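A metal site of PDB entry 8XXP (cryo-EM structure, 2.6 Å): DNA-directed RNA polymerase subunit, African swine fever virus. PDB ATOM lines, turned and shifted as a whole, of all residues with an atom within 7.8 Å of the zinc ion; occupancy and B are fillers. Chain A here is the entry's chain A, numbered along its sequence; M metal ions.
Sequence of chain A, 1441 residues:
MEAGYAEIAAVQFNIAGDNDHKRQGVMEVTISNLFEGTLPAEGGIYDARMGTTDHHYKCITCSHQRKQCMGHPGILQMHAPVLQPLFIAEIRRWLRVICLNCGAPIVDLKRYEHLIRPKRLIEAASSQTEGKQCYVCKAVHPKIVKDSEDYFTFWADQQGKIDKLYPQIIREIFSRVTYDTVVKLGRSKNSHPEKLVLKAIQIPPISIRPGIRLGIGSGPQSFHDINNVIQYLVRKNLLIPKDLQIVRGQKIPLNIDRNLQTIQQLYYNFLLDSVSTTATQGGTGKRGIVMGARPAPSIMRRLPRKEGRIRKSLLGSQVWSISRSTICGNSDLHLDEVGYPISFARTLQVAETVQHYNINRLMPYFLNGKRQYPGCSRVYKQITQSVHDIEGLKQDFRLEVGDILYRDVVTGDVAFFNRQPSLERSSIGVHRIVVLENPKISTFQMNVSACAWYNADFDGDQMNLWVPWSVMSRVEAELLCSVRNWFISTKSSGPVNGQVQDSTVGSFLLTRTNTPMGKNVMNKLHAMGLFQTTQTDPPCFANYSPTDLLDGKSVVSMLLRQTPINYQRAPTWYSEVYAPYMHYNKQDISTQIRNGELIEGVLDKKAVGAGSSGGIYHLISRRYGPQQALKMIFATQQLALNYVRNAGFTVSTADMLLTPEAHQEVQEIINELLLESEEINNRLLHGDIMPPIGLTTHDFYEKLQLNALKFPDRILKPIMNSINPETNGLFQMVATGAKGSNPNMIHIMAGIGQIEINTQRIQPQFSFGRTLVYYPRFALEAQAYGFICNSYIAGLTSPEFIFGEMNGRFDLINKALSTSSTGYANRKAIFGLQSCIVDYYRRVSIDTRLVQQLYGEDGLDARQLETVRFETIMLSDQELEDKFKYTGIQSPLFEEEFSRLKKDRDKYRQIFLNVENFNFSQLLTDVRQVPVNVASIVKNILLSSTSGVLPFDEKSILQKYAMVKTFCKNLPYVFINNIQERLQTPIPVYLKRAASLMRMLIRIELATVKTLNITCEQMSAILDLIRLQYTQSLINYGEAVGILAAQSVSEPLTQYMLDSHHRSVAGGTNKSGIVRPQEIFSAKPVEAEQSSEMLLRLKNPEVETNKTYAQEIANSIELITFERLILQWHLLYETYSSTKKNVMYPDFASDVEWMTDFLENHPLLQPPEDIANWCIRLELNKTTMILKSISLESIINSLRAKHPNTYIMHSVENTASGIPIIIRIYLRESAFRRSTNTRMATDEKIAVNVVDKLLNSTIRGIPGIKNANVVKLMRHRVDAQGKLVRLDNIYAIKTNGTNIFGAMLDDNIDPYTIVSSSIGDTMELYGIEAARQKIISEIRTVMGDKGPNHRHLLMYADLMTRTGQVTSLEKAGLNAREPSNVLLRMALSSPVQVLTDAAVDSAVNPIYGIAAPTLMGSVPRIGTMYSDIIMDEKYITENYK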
ATOM      1  N   ILE A  98     -10.648   0.452  -2.806  1.00  0.00           N
ATOM      2  CA  ILE A  98     -12.047   0.043  -2.786  1.00  0.00           C
ATOM      3  C   ILE A  98     -12.139  -1.406  -2.363  1.00  0.00           C
ATOM      4  O   ILE A  98     -11.324  -2.239  -2.789  1.00  0.00           O
ATOM      5  CB  ILE A  98     -12.705   0.273  -4.166  1.00  0.00           C
ATOM      6  CG1 ILE A  98     -12.828   1.764  -4.446  1.00  0.00           C
ATOM      7  CG2 ILE A  98     -14.067  -0.388  -4.229  1.00  0.00           C
ATOM      8  CD1 ILE A  98     -13.960   2.436  -3.723  1.00  0.00           C
ATOM      9  N   CYS A  99     -13.110  -1.709  -1.507  1.00  0.00           N
ATOM     10  CA  CYS A  99     -13.406  -3.109  -1.186  1.00  0.00           C
ATOM     11  C   CYS A  99     -13.945  -3.816  -2.417  1.00  0.00           C
ATOM     12  O   CYS A  99     -14.810  -3.291  -3.122  1.00  0.00           O
ATOM     13  CB  CYS A  99     -14.416  -3.180  -0.055  1.00  0.00           C
ATOM     14  SG  CYS A  99     -15.044  -4.853   0.227  1.00  0.00           S
ATOM     15  N   LEU A 100     -13.433  -5.021  -2.671  1.00  0.00           N
ATOM     16  CA  LEU A 100     -13.824  -5.747  -3.871  1.00  0.00           C
ATOM     17  C   LEU A 100     -15.214  -6.362  -3.715  1.00  0.00           C
ATOM     18  O   LEU A 100     -15.950  -6.489  -4.698  1.00  0.00           O
ATOM     19  CB  LEU A 100     -12.789  -6.808  -4.195  1.00  0.00           C
ATOM     20  CG  LEU A 100     -11.349  -6.303  -4.295  1.00  0.00           C
ATOM     21  CD1 LEU A 100     -10.453  -7.332  -4.952  1.00  0.00           C
ATOM     22  CD2 LEU A 100     -11.292  -5.000  -5.070  1.00  0.00           C
ATOM     23  N   ASN A 101     -15.587  -6.744  -2.495  1.00  0.00           N
ATOM     24  CA  ASN A 101     -16.826  -7.488  -2.315  1.00  0.00           C
ATOM     25  C   ASN A 101     -18.054  -6.597  -2.407  1.00  0.00           C
ATOM     26  O   ASN A 101     -19.080  -7.008  -2.962  1.00  0.00           O
ATOM     27  CB  ASN A 101     -16.806  -8.225  -0.975  1.00  0.00           C
ATOM     28  CG  ASN A 101     -16.413  -9.681  -1.113  1.00  0.00           C
ATOM     29  OD1 ASN A 101     -15.535 -10.015  -1.918  1.00  0.00           O
ATOM     30  ND2 ASN A 101     -17.056 -10.544  -0.353  1.00  0.00           N
ATOM     31  N   CYS A 102     -17.985  -5.376  -1.879  1.00  0.00           N
ATOM     32  CA  CYS A 102     -19.157  -4.507  -1.838  1.00  0.00           C
ATOM     33  C   CYS A 102     -18.936  -3.107  -2.378  1.00  0.00           C
ATOM     34  O   CYS A 102     -19.907  -2.356  -2.488  1.00  0.00           O
ATOM     35  CB  CYS A 102     -19.695  -4.391  -0.403  1.00  0.00           C
ATOM     36  SG  CYS A 102     -18.634  -3.468   0.715  1.00  0.00           S
ATOM     37  N   GLY A 103     -17.703  -2.725  -2.711  1.00  0.00           N
ATOM     38  CA  GLY A 103     -17.442  -1.439  -3.310  1.00  0.00           C
ATOM     39  C   GLY A 103     -17.290  -0.290  -2.342  1.00  0.00           C
ATOM     40  O   GLY A 103     -17.003   0.830  -2.779  1.00  0.00           O
ATOM     41  N   ALA A 104     -17.463  -0.519  -1.045  1.00  0.00           N
ATOM     42  CA  ALA A 104     -17.262   0.537  -0.080  1.00  0.00           C
ATOM     43  C   ALA A 104     -15.777   0.874   0.039  1.00  0.00           C
ATOM     44  O   ALA A 104     -14.921   0.006  -0.150  1.00  0.00           O
ATOM     45  CB  ALA A 104     -17.817   0.138   1.278  1.00  0.00           C
ATOM     46  N   PRO A 105     -15.444   2.126   0.347  1.00  0.00           N
ATOM     47  CA  PRO A 105     -14.030   2.481   0.519  1.00  0.00           C
ATOM     48  C   PRO A 105     -13.462   1.831   1.773  1.00  0.00           C
ATOM     49  O   PRO A 105     -14.010   1.985   2.861  1.00  0.00           O
ATOM     50  CB  PRO A 105     -14.059   4.004   0.639  1.00  0.00           C
ATOM     51  CG  PRO A 105     -15.428   4.307   1.128  1.00  0.00           C
ATOM     52  CD  PRO A 105     -16.334   3.278   0.543  1.00  0.00           C
ATOM     53  N   ILE A 106     -12.363   1.089   1.608  1.00  0.00           N
ATOM     54  CA  ILE A 106     -11.723   0.505   2.766  1.00  0.00           C
ATOM     55  C   ILE A 106     -10.953   1.547   3.574  1.00  0.00           C
ATOM     56  O   ILE A 106     -10.759   1.367   4.779  1.00  0.00           O
ATOM     57  CB  ILE A 106     -10.787  -0.652   2.378  1.00  0.00           C
ATOM     58  CG1 ILE A 106      -9.818  -0.220   1.287  1.00  0.00           C
ATOM     59  CG2 ILE A 106     -11.600  -1.849   1.924  1.00  0.00           C
ATOM     60  CD1 ILE A 106      -8.642  -1.139   1.150  1.00  0.00           C
ATOM     61  N   GLN A 133      -9.797  -4.740   6.935  1.00  0.00           N
ATOM     62  CA  GLN A 133     -11.108  -5.356   7.008  1.00  0.00           C
ATOM     63  C   GLN A 133     -12.171  -4.333   6.646  1.00  0.00           C
ATOM     64  O   GLN A 133     -12.202  -3.240   7.223  1.00  0.00           O
ATOM     65  CB  GLN A 133     -11.375  -5.922   8.400  1.00  0.00           C
ATOM     66  CG  GLN A 133     -12.264  -7.154   8.417  1.00  0.00           C
ATOM     67  CD  GLN A 133     -13.303  -7.111   9.521  1.00  0.00           C
ATOM     68  OE1 GLN A 133     -13.546  -6.069  10.122  1.00  0.00           O
ATOM     69  NE2 GLN A 133     -13.922  -8.256   9.782  1.00  0.00           N
ATOM     70  N   CYS A 134     -13.030  -4.685   5.698  1.00  0.00           N
ATOM     71  CA  CYS A 134     -14.120  -3.795   5.314  1.00  0.00           C
ATOM     72  C   CYS A 134     -15.125  -3.664   6.448  1.00  0.00           C
ATOM     73  O   CYS A 134     -15.435  -4.630   7.140  1.00  0.00           O
ATOM     74  CB  CYS A 134     -14.796  -4.298   4.049  1.00  0.00           C
ATOM     75  SG  CYS A 134     -16.247  -3.351   3.555  1.00  0.00           S
ATOM     76  N   TYR A 135     -15.635  -2.448   6.632  1.00  0.00           N
ATOM     77  CA  TYR A 135     -16.647  -2.233   7.659  1.00  0.00           C
ATOM     78  C   TYR A 135     -17.973  -2.880   7.265  1.00  0.00           C
ATOM     79  O   TYR A 135     -18.600  -3.570   8.087  1.00  0.00           O
ATOM     80  CB  TYR A 135     -16.814  -0.730   7.911  1.00  0.00           C
ATOM     81  CG  TYR A 135     -17.562  -0.333   9.174  1.00  0.00           C
ATOM     82  CD1 TYR A 135     -17.137   0.743   9.937  1.00  0.00           C
ATOM     83  CD2 TYR A 135     -18.700  -1.016   9.603  1.00  0.00           C
ATOM     84  CE1 TYR A 135     -17.803   1.123  11.093  1.00  0.00           C
ATOM     85  CE2 TYR A 135     -19.377  -0.649  10.749  1.00  0.00           C
ATOM     86  CZ  TYR A 135     -18.921   0.419  11.488  1.00  0.00           C
ATOM     87  OH  TYR A 135     -19.598   0.787  12.635  1.00  0.00           O
ATOM     88  N   VAL A 136     -18.413  -2.673   6.031  1.00  0.00           N
ATOM     89  CA  VAL A 136     -19.754  -3.099   5.640  1.00  0.00           C
ATOM     90  C   VAL A 136     -19.844  -4.615   5.545  1.00  0.00           C
ATOM     91  O   VAL A 136     -20.784  -5.231   6.077  1.00  0.00           O
ATOM     92  CB  VAL A 136     -20.162  -2.423   4.317  1.00  0.00           C
ATOM     93  CG1 VAL A 136     -21.530  -2.889   3.871  1.00  0.00           C
ATOM     94  CG2 VAL A 136     -20.143  -0.910   4.472  1.00  0.00           C
ATOM     95  N   CYS A 137     -18.883  -5.253   4.871  1.00  0.00           N
ATOM     96  CA  CYS A 137     -18.996  -6.672   4.559  1.00  0.00           C
ATOM     97  C   CYS A 137     -17.910  -7.520   5.196  1.00  0.00           C
ATOM     98  O   CYS A 137     -17.834  -8.727   4.923  1.00  0.00           O
ATOM     99  CB  CYS A 137     -19.000  -6.883   3.047  1.00  0.00           C
ATOM    100  SG  CYS A 137     -17.368  -6.773   2.270  1.00  0.00           S
ATOM    101  N   LYS A 138     -17.060  -6.931   6.049  1.00  0.00           N
ATOM    102  CA  LYS A 138     -16.067  -7.650   6.839  1.00  0.00           C
ATOM    103  C   LYS A 138     -15.095  -8.465   5.987  1.00  0.00           C
ATOM    104  O   LYS A 138     -14.526  -9.455   6.462  1.00  0.00           O
ATOM    105  CB  LYS A 138     -16.726  -8.569   7.885  1.00  0.00           C
ATOM    106  CG  LYS A 138     -18.047  -8.049   8.445  1.00  0.00           C
ATOM    107  CD  LYS A 138     -17.884  -7.472   9.852  1.00  0.00           C
ATOM    108  CE  LYS A 138     -17.317  -6.058   9.818  1.00  0.00           C
ATOM    109  NZ  LYS A 138     -17.345  -5.418  11.152  1.00  0.00           N
ATOM    110  N   ALA A 139     -14.879  -8.084   4.730  1.00  0.00           N
ATOM    111  CA  ALA A 139     -13.973  -8.805   3.858  1.00  0.00           C
ATOM    112  C   ALA A 139     -12.576  -8.210   3.940  1.00  0.00           C
ATOM    113  O   ALA A 139     -12.415  -6.981   3.993  1.00  0.00           O
ATOM    114  CB  ALA A 139     -14.459  -8.785   2.424  1.00  0.00           C
ATOM    115  N   VAL A 140     -11.574  -9.075   3.944  1.00  0.00           N
ATOM    116  CA  VAL A 140     -10.186  -8.646   4.004  1.00  0.00           C
ATOM    117  C   VAL A 140      -9.731  -8.239   2.614  1.00  0.00           C
ATOM    118  O   VAL A 140      -9.836  -9.027   1.664  1.00  0.00           O
ATOM    119  CB  VAL A 140      -9.296  -9.757   4.575  1.00  0.00           C
ATOM    120  CG1 VAL A 140      -7.834  -9.374   4.479  1.00  0.00           C
ATOM    121  CG2 VAL A 140      -9.682 -10.046   6.018  1.00  0.00           C
HETATM  122 ZN    ZN M   1     -16.834  -4.584   1.681  1.00  0.00          ZN
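SG of Cys 102 lies close to N of Ala 104, 3.6 Å away. The backbone NH of Cys 134 is in hydrogen-bond range of the backbone carbonyl oxygen of Ala 139, at 2.9 Å. The backbone NH (N) of Cys 99 lies within hydrogen-bond range of the backbone carbonyl oxygen (O) of Ala 104, 2.8 Å away. The side-chain sulfur (SG) of Cys 99 sits close to the backbone NH (N) of Asn 101 (3.4 Å). The side-chain sulfur (SG) of Cys 137 lies close to the backbone NH (N) of Ala 139 (3.7 Å). The side-chain sulfur (SG) of Cys 134 sits close to the backbone NH (N) of Val 136, at 3.4 Å.
Within 4 Å of the zinc ion: Cys 99, Cys 102, Cys 134 and Cys 137. The nearest printed residue that does not touch the zinc ion is Asn 101 (4.5 Å).
SG of Cys 134 is bound to the zinc ion (2.3 Å). SG of Cys 99 is bound to the zinc ion (2.3 Å). SG of Cys 102 is bound to the zinc ion. The zinc ion is bound by SG of Cys 137 (2.3 Å). The zinc ion has four donor atoms within binding distance.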
